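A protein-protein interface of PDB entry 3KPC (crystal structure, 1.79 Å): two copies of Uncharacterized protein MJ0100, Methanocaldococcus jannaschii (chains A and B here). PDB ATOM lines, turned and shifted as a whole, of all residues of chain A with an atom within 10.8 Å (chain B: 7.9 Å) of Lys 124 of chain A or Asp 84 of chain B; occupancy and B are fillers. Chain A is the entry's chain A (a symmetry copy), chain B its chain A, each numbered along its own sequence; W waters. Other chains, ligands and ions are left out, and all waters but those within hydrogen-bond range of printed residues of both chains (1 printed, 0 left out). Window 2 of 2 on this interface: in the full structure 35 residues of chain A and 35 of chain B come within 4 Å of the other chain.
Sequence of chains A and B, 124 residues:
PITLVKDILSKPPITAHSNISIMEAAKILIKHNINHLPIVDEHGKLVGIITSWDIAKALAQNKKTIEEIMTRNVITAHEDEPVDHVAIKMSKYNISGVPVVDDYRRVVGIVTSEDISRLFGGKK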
ATOM      1  N   ILE A 116     -26.146  -9.032  18.567  1.00  0.00           N
ATOM      2  CA  ILE A 116     -25.216  -8.350  19.462  1.00  0.00           C
ATOM      3  C   ILE A 116     -25.098  -6.877  19.090  1.00  0.00           C
ATOM      4  O   ILE A 116     -25.046  -6.006  19.968  1.00  0.00           O
ATOM      5  CB  ILE A 116     -23.838  -9.048  19.475  1.00  0.00           C
ATOM      6  CG1 ILE A 116     -24.008 -10.506  19.941  1.00  0.00           C
ATOM      7  CG2 ILE A 116     -22.839  -8.280  20.353  1.00  0.00           C
ATOM      8  CD1 ILE A 116     -22.725 -11.232  20.293  1.00  0.00           C
ATOM      9  N   SER A 117     -25.085  -6.598  17.787  1.00  0.00           N
ATOM     10  CA  SER A 117     -25.057  -5.225  17.293  1.00  0.00           C
ATOM     11  C   SER A 117     -26.313  -4.472  17.733  1.00  0.00           C
ATOM     12  O   SER A 117     -26.240  -3.293  18.089  1.00  0.00           O
ATOM     13  CB  SER A 117     -24.915  -5.198  15.768  1.00  0.00           C
ATOM     14  OG  SER A 117     -24.841  -3.872  15.283  1.00  0.00           O
ATOM     15  N   ARG A 118     -27.454  -5.159  17.711  1.00  0.00           N
ATOM     16  CA  ARG A 118     -28.721  -4.590  18.174  1.00  0.00           C
ATOM     17  C   ARG A 118     -28.638  -4.238  19.652  1.00  0.00           C
ATOM     18  O   ARG A 118     -29.117  -3.179  20.075  1.00  0.00           O
ATOM     19  CB  ARG A 118     -29.869  -5.578  17.945  1.00  0.00           C
ATOM     20  CG  ARG A 118     -31.248  -5.087  18.393  1.00  0.00           C
ATOM     21  CD  ARG A 118     -32.331  -6.135  18.142  1.00  0.00           C
ATOM     22  NE  ARG A 118     -32.276  -6.651  16.774  1.00  0.00           N
ATOM     23  CZ  ARG A 118     -31.877  -7.877  16.438  1.00  0.00           C
ATOM     24  NH1 ARG A 118     -31.517  -8.750  17.371  1.00  0.00           N
ATOM     25  NH2 ARG A 118     -31.859  -8.236  15.159  1.00  0.00           N
ATOM     26  N   LEU A 119     -28.042  -5.140  20.429  1.00  0.00           N
ATOM     27  CA  LEU A 119     -27.860  -4.944  21.857  1.00  0.00           C
ATOM     28  C   LEU A 119     -27.000  -3.707  22.106  1.00  0.00           C
ATOM     29  O   LEU A 119     -27.337  -2.875  22.947  1.00  0.00           O
ATOM     30  CB  LEU A 119     -27.229  -6.191  22.486  1.00  0.00           C
ATOM     31  CG  LEU A 119     -27.204  -6.321  24.013  1.00  0.00           C
ATOM     32  CD1 LEU A 119     -28.616  -6.373  24.583  1.00  0.00           C
ATOM     33  CD2 LEU A 119     -26.435  -7.571  24.410  1.00  0.00           C
ATOM     34  N   PHE A 120     -25.913  -3.580  21.345  1.00  0.00           N
ATOM     35  CA  PHE A 120     -25.030  -2.413  21.403  1.00  0.00           C
ATOM     36  C   PHE A 120     -25.781  -1.096  21.185  1.00  0.00           C
ATOM     37  O   PHE A 120     -25.499  -0.101  21.855  1.00  0.00           O
ATOM     38  CB  PHE A 120     -23.904  -2.552  20.371  1.00  0.00           C
ATOM     39  CG  PHE A 120     -22.900  -1.427  20.396  1.00  0.00           C
ATOM     40  CD1 PHE A 120     -21.748  -1.529  21.167  1.00  0.00           C
ATOM     41  CD2 PHE A 120     -23.097  -0.276  19.634  1.00  0.00           C
ATOM     42  CE1 PHE A 120     -20.810  -0.498  21.191  1.00  0.00           C
ATOM     43  CE2 PHE A 120     -22.168   0.761  19.653  1.00  0.00           C
ATOM     44  CZ  PHE A 120     -21.024   0.649  20.434  1.00  0.00           C
ATOM     45  N   GLY A 121     -26.731  -1.100  20.252  1.00  0.00           N
ATOM     46  CA  GLY A 121     -27.458   0.115  19.881  1.00  0.00           C
ATOM     47  C   GLY A 121     -28.528   0.565  20.862  1.00  0.00           C
ATOM     48  O   GLY A 121     -28.804   1.759  20.974  1.00  0.00           O
ATOM     49  N   GLY A 122     -29.129  -0.394  21.569  1.00  0.00           N
ATOM     50  CA  GLY A 122     -30.229  -0.118  22.508  1.00  0.00           C
ATOM     51  C   GLY A 122     -29.750   0.201  23.913  1.00  0.00           C
ATOM     52  O   GLY A 122     -30.451   0.858  24.695  1.00  0.00           O
ATOM     53  N   LYS A 123     -28.558  -0.300  24.231  1.00  0.00           N
ATOM     54  CA  LYS A 123     -27.775   0.171  25.363  1.00  0.00           C
ATOM     55  C   LYS A 123     -27.522   1.659  25.161  1.00  0.00           C
ATOM     56  O   LYS A 123     -27.597   2.452  26.105  1.00  0.00           O
ATOM     57  CB  LYS A 123     -26.429  -0.565  25.427  1.00  0.00           C
ATOM     58  CG  LYS A 123     -26.368  -1.776  26.377  1.00  0.00           C
ATOM     59  CD  LYS A 123     -27.213  -2.954  25.869  1.00  0.00           C
ATOM     60  CE  LYS A 123     -27.478  -3.957  26.977  1.00  0.00           C
ATOM     61  NZ  LYS A 123     -28.562  -3.499  27.896  1.00  0.00           N
ATOM     62  N   LYS A 124     -27.250   2.014  23.901  1.00  0.00           N
ATOM     63  CA  LYS A 124     -26.589   3.269  23.525  1.00  0.00           C
ATOM     64  C   LYS A 124     -25.323   3.473  24.364  1.00  0.00           C
ATOM     65  O   LYS A 124     -24.722   2.508  24.851  1.00  0.00           O
ATOM     66  CB  LYS A 124     -27.535   4.481  23.630  1.00  0.00           C
ATOM     67  CG  LYS A 124     -28.548   4.629  22.501  1.00  0.00           C
ATOM     68  CD  LYS A 124     -29.349   5.931  22.691  1.00  0.00           C
ATOM     69  CE  LYS A 124     -30.281   6.202  21.516  1.00  0.00           C
ATOM     70  NZ  LYS A 124     -31.467   5.281  21.498  1.00  0.00           N
ATOM     71  OXT LYS A 124     -24.858   4.594  24.584  1.00  0.00           O
ATOM     72  N   PRO B   1     -15.805   7.680  26.089  1.00  0.00           N
ATOM     73  CA  PRO B   1     -15.831   8.535  24.898  1.00  0.00           C
ATOM     74  C   PRO B   1     -16.984   8.156  23.958  1.00  0.00           C
ATOM     75  O   PRO B   1     -17.664   7.157  24.203  1.00  0.00           O
ATOM     76  CB  PRO B   1     -14.478   8.245  24.225  1.00  0.00           C
ATOM     77  CG  PRO B   1     -13.688   7.408  25.210  1.00  0.00           C
ATOM     78  CD  PRO B   1     -14.705   6.703  26.044  1.00  0.00           C
ATOM     79  N   ILE B   2     -17.216   8.937  22.903  1.00  0.00           N
ATOM     80  CA  ILE B   2     -18.166   8.526  21.863  1.00  0.00           C
ATOM     81  C   ILE B   2     -17.395   7.933  20.677  1.00  0.00           C
ATOM     82  O   ILE B   2     -16.602   8.630  20.039  1.00  0.00           O
ATOM     83  CB  ILE B   2     -19.088   9.690  21.394  1.00  0.00           C
ATOM     84  CG1 ILE B   2     -19.849  10.292  22.583  1.00  0.00           C
ATOM     85  CG2 ILE B   2     -20.056   9.207  20.306  1.00  0.00           C
ATOM     86  CD1 ILE B   2     -20.565  11.613  22.267  1.00  0.00           C
ATOM     87  N   THR B   3     -17.616   6.649  20.397  1.00  0.00           N
ATOM     88  CA  THR B   3     -16.955   5.972  19.276  1.00  0.00           C
ATOM     89  C   THR B   3     -17.648   6.348  17.972  1.00  0.00           C
ATOM     90  O   THR B   3     -18.877   6.294  17.884  1.00  0.00           O
ATOM     91  CB  THR B   3     -16.968   4.434  19.451  1.00  0.00           C
ATOM     92  OG1 THR B   3     -16.432   4.091  20.735  1.00  0.00           O
ATOM     93  CG2 THR B   3     -16.142   3.749  18.365  1.00  0.00           C
ATOM     94  N   LEU B   4     -16.867   6.733  16.968  1.00  0.00           N
ATOM     95  CA  LEU B   4     -17.428   7.118  15.677  1.00  0.00           C
ATOM     96  C   LEU B   4     -17.095   6.090  14.614  1.00  0.00           C
ATOM     97  O   LEU B   4     -16.195   5.265  14.797  1.00  0.00           O
ATOM     98  CB  LEU B   4     -16.920   8.504  15.261  1.00  0.00           C
ATOM     99  CG  LEU B   4     -17.091   9.639  16.276  1.00  0.00           C
ATOM    100  CD1 LEU B   4     -16.476  10.925  15.754  1.00  0.00           C
ATOM    101  CD2 LEU B   4     -18.553   9.867  16.653  1.00  0.00           C
ATOM    102  N   VAL B   5     -17.833   6.136  13.507  1.00  0.00           N
ATOM    103  CA  VAL B   5     -17.618   5.227  12.382  1.00  0.00           C
ATOM    104  C   VAL B   5     -16.156   5.204  11.945  1.00  0.00           C
ATOM    105  O   VAL B   5     -15.588   4.128  11.734  1.00  0.00           O
ATOM    106  CB  VAL B   5     -18.535   5.575  11.183  1.00  0.00           C
ATOM    107  CG1 VAL B   5     -18.021   4.968   9.879  1.00  0.00           C
ATOM    108  CG2 VAL B   5     -19.958   5.120  11.455  1.00  0.00           C
ATOM    109  N   ILE B   8     -13.759   2.735  13.667  1.00  0.00           N
ATOM    110  CA  ILE B   8     -13.908   1.270  13.531  1.00  0.00           C
ATOM    111  C   ILE B   8     -14.102   0.719  12.113  1.00  0.00           C
ATOM    112  O   ILE B   8     -14.090  -0.503  11.920  1.00  0.00           O
ATOM    113  CB  ILE B   8     -15.057   0.700  14.421  1.00  0.00           C
ATOM    114  CG1 ILE B   8     -16.440   1.108  13.872  1.00  0.00           C
ATOM    115  CG2 ILE B   8     -14.868   1.096  15.887  1.00  0.00           C
ATOM    116  CD1 ILE B   8     -17.563   0.126  14.301  1.00  0.00           C
ATOM    117  N   GLU B  81     -20.294   9.735  12.057  1.00  0.00           N
ATOM    118  CA  GLU B  81     -21.498   9.241  12.704  1.00  0.00           C
ATOM    119  C   GLU B  81     -21.135   8.385  13.916  1.00  0.00           C
ATOM    120  O   GLU B  81     -20.235   7.544  13.827  1.00  0.00           O
ATOM    121  CB  GLU B  81     -22.316   8.437  11.696  1.00  0.00           C
ATOM    122  CG  GLU B  81     -23.713   8.058  12.156  1.00  0.00           C
ATOM    123  CD  GLU B  81     -24.583   7.583  11.010  1.00  0.00           C
ATOM    124  OE1 GLU B  81     -24.171   7.717   9.837  1.00  0.00           O
ATOM    125  OE2 GLU B  81     -25.695   7.084  11.281  1.00  0.00           O
ATOM    126  N   PRO B  82     -21.814   8.610  15.061  1.00  0.00           N
ATOM    127  CA  PRO B  82     -21.626   7.723  16.209  1.00  0.00           C
ATOM    128  C   PRO B  82     -21.994   6.287  15.854  1.00  0.00           C
ATOM    129  O   PRO B  82     -23.025   6.055  15.214  1.00  0.00           O
ATOM    130  CB  PRO B  82     -22.606   8.283  17.245  1.00  0.00           C
ATOM    131  CG  PRO B  82     -22.714   9.726  16.900  1.00  0.00           C
ATOM    132  CD  PRO B  82     -22.667   9.765  15.398  1.00  0.00           C
ATOM    133  N   VAL B  83     -21.153   5.340  16.263  1.00  0.00           N
ATOM    134  CA  VAL B  83     -21.366   3.924  15.960  1.00  0.00           C
ATOM    135  C   VAL B  83     -22.714   3.425  16.492  1.00  0.00           C
ATOM    136  O   VAL B  83     -23.356   2.587  15.846  1.00  0.00           O
ATOM    137  CB  VAL B  83     -20.193   3.035  16.464  1.00  0.00           C
ATOM    138  CG1 VAL B  83     -20.504   1.548  16.297  1.00  0.00           C
ATOM    139  CG2 VAL B  83     -18.909   3.383  15.719  1.00  0.00           C
ATOM    140  N   ASP B  84     -23.159   3.943  17.640  1.00  0.00           N
ATOM    141  CA  ASP B  84     -24.458   3.511  18.166  1.00  0.00           C
ATOM    142  C   ASP B  84     -25.646   3.935  17.285  1.00  0.00           C
ATOM    143  O   ASP B  84     -26.629   3.197  17.196  1.00  0.00           O
ATOM    144  CB  ASP B  84     -24.660   3.860  19.659  1.00  0.00           C
ATOM    145  CG  ASP B  84     -24.864   5.349  19.910  1.00  0.00           C
ATOM    146  OD1 ASP B  84     -24.362   6.180  19.124  1.00  0.00           O
ATOM    147  OD2 ASP B  84     -25.530   5.686  20.919  1.00  0.00           O
ATOM    148  N   HIS B  85     -25.553   5.094  16.626  1.00  0.00           N
ATOM    149  CA  HIS B  85     -26.582   5.531  15.662  1.00  0.00           C
ATOM    150  C   HIS B  85     -26.687   4.535  14.507  1.00  0.00           C
ATOM    151  O   HIS B  85     -27.783   4.234  14.023  1.00  0.00           O
ATOM    152  CB  HIS B  85     -26.257   6.921  15.099  1.00  0.00           C
ATOM    153  CG  HIS B  85     -26.405   8.041  16.085  1.00  0.00           C
ATOM    154  ND1 HIS B  85     -26.427   7.844  17.450  1.00  0.00           N
ATOM    155  CD2 HIS B  85     -26.503   9.381  15.901  1.00  0.00           C
ATOM    156  CE1 HIS B  85     -26.548   9.009  18.062  1.00  0.00           C
ATOM    157  NE2 HIS B  85     -26.596   9.958  17.144  1.00  0.00           N
ATOM    158  N   VAL B  86     -25.527   4.034  14.080  1.00  0.00           N
ATOM    159  CA  VAL B  86     -25.427   3.054  13.000  1.00  0.00           C
ATOM    160  C   VAL B  86     -26.029   1.716  13.422  1.00  0.00           C
ATOM    161  O   VAL B  86     -26.781   1.109  12.660  1.00  0.00           O
ATOM    162  CB  VAL B  86     -23.960   2.865  12.537  1.00  0.00           C
ATOM    163  CG1 VAL B  86     -23.848   1.749  11.504  1.00  0.00           C
ATOM    164  CG2 VAL B  86     -23.412   4.169  11.975  1.00  0.00           C
ATOM    165  N   ALA B  87     -25.701   1.265  14.633  1.00  0.00           N
ATOM    166  CA  ALA B  87     -26.290   0.037  15.179  1.00  0.00           C
ATOM    167  C   ALA B  87     -27.822   0.095  15.209  1.00  0.00           C
ATOM    168  O   ALA B  87     -28.491  -0.874  14.836  1.00  0.00           O
ATOM    169  CB  ALA B  87     -25.732  -0.253  16.566  1.00  0.00           C
ATOM    170  N   ILE B  88     -28.369   1.227  15.648  1.00  0.00           N
ATOM    171  CA  ILE B  88     -29.821   1.422  15.700  1.00  0.00           C
ATOM    172  C   ILE B  88     -30.425   1.372  14.292  1.00  0.00           C
ATOM    173  O   ILE B  88     -31.494   0.793  14.086  1.00  0.00           O
ATOM    174  CB  ILE B  88     -30.191   2.750  16.416  1.00  0.00           C
ATOM    175  CG1 ILE B  88     -29.865   2.659  17.913  1.00  0.00           C
ATOM    176  CG2 ILE B  88     -31.672   3.098  16.221  1.00  0.00           C
ATOM    177  CD1 ILE B  88     -29.641   4.001  18.586  1.00  0.00           C
ATOM    178  N   LYS B  89     -29.719   1.970  13.335  1.00  0.00           N
ATOM    179  CA  LYS B  89     -30.124   2.000  11.935  1.00  0.00           C
ATOM    180  C   LYS B  89     -30.198   0.598  11.347  1.00  0.00           C
ATOM    181  O   LYS B  89     -31.191   0.232  10.710  1.00  0.00           O
ATOM    182  CB  LYS B  89     -29.109   2.829  11.154  1.00  0.00           C
ATOM    183  CG  LYS B  89     -29.716   3.758  10.125  1.00  0.00           C
ATOM    184  CD  LYS B  89     -28.941   5.075  10.069  1.00  0.00           C
ATOM    185  CE  LYS B  89     -27.588   4.902   9.371  1.00  0.00           C
ATOM    186  NZ  LYS B  89     -26.977   6.221   9.017  1.00  0.00           N
ATOM    187  N   MET B  90     -29.143  -0.184  11.569  1.00  0.00           N
ATOM    188  CA  MET B  90     -29.079  -1.555  11.072  1.00  0.00           C
ATOM    189  C   MET B  90     -30.182  -2.420  11.678  1.00  0.00           C
ATOM    190  O   MET B  90     -30.757  -3.260  10.987  1.00  0.00           O
ATOM    191  CB  MET B  90     -27.706  -2.172  11.336  1.00  0.00           C
ATOM    192  CG  MET B  90     -26.566  -1.476  10.602  1.00  0.00           C
ATOM    193  SD  MET B  90     -25.027  -2.439  10.577  1.00  0.00           S
ATOM    194  CE  MET B  90     -24.929  -2.980  12.282  1.00  0.00           C
ATOM    195  N   SER B  91     -30.472  -2.212  12.960  1.00  0.00           N
ATOM    196  CA  SER B  91     -31.547  -2.943  13.623  1.00  0.00           C
ATOM    197  C   SER B  91     -32.913  -2.538  13.069  1.00  0.00           C
ATOM    198  O   SER B  91     -33.754  -3.401  12.791  1.00  0.00           O
ATOM    199  CB  SER B  91     -31.499  -2.733  15.136  1.00  0.00           C
ATOM    200  OG  SER B  91     -32.517  -3.495  15.787  1.00  0.00           O
ATOM    201  N   ILE B 116     -19.437  -4.041  14.833  1.00  0.00           N
ATOM    202  CA  ILE B 116     -20.124  -3.504  16.005  1.00  0.00           C
ATOM    203  C   ILE B 116     -20.152  -4.537  17.126  1.00  0.00           C
ATOM    204  O   ILE B 116     -19.961  -4.198  18.302  1.00  0.00           O
ATOM    205  CB  ILE B 116     -21.543  -3.009  15.647  1.00  0.00           C
ATOM    206  CG1 ILE B 116     -21.444  -1.909  14.574  1.00  0.00           C
ATOM    207  CG2 ILE B 116     -22.289  -2.524  16.898  1.00  0.00           C
ATOM    208  CD1 ILE B 116     -22.713  -1.118  14.334  1.00  0.00           C
ATOM    209  N   LEU B 119     -16.859  -4.531  18.746  1.00  0.00           N
ATOM    210  CA  LEU B 119     -16.768  -3.371  19.618  1.00  0.00           C
ATOM    211  C   LEU B 119     -17.440  -3.675  20.956  1.00  0.00           C
ATOM    212  O   LEU B 119     -16.878  -3.389  22.012  1.00  0.00           O
ATOM    213  CB  LEU B 119     -17.405  -2.152  18.944  1.00  0.00           C
ATOM    214  CG  LEU B 119     -17.176  -0.764  19.553  1.00  0.00           C
ATOM    215  CD1 LEU B 119     -15.700  -0.390  19.530  1.00  0.00           C
ATOM    216  CD2 LEU B 119     -17.989   0.271  18.791  1.00  0.00           C
HETATM  217  O   HOH W   1     -27.496  -3.351  14.768  1.00  0.00           O
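OG of Ser 91 of chain B sits close to NE of Arg 118 of chain A (3.3 Å).
OD1 of Asp 84 of chain B is in hydrogen-bond range of ND1 of His 85 of chain B, 3.1 Å away.
O of Thr 3 of chain B lies within hydrogen-bond range of N of Val 83 of chain B.
Among the printed residues, merely in contact across the chains: Ser 117 of chain A with Met 90 of chain B, Ser 117 of chain A with Ile 116 of chain B, Gly 121 of chain A with Ile 88 of chain B, Ser 117 of chain A with Ala 87 of chain B, Phe 120 of chain A with Leu 119 of chain B, Lys 124 of chain A with Asp 84 of chain B, Phe 120 of chain A with Ile 116 of chain B, Lys 124 of chain A with Ile 88 of chain B, Gly 121 of chain A with Ala 87 of chain B, Phe 120 of chain A with Val 83 of chain B and Phe 120 of chain A with Asp 84 of chain B.
Printed residues of chain B within 4 Å of Lys 124 of chain A: Asp 84 and Ile 88.
Asp 84 of chain B touches just these residues of chain A: Phe 120 and Lys 124.
Val 86 of chain B touches none of the printed residues of chain A.
Of the printed residues of chain A, Ser 91 of chain B touches Arg 118.
Printed residues of chain A within 4 Å of Met 90 of chain B: Ser 117 (3.1 Å).
Of the printed residues of chain B, Ser 117 of chain A touches Ala 87 (3.4 Å), Met 90 (3.1 Å) and Ile 116 (3.3 Å).
Printed residues of chain A within 4 Å of Leu 119 of chain B: Phe 120 (3.5 Å).
Thr 3 of chain B touches none of the printed residues of chain A.
The nearest residue of chain B that does not touch Lys 124 of chain A is His 85 of chain B (5.8 Å).
The nearest printed residue of chain A that does not touch Leu 119 of chain B is Ile 116 of chain A (7.1 Å).
Of the 19 printed residues of chain B, 8 touch a printed residue of chain A.
Hydrophobic or aromatic side chains of chain A that line the printed part of chain B: Phe 120.
Among the printed residues, 12 pairs touch across the chains.
Among the printed residues, no Asp or Glu carboxylate lies within 4 Å of a Lys or Arg side-chain nitrogen of the other chain.
Positions printed for both chains: 116 and 119.
Of the 12 pairs that touch across the chains among the printed residues, none has its exchanged pair printed and touching as well.
Water W1 lies within hydrogen-bond range of O of Ala 87 of chain B (2.7 Å), OG of Ser 117 of chain A (2.8 Å) and N of Arg 118 of chain A (3.5 Å).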
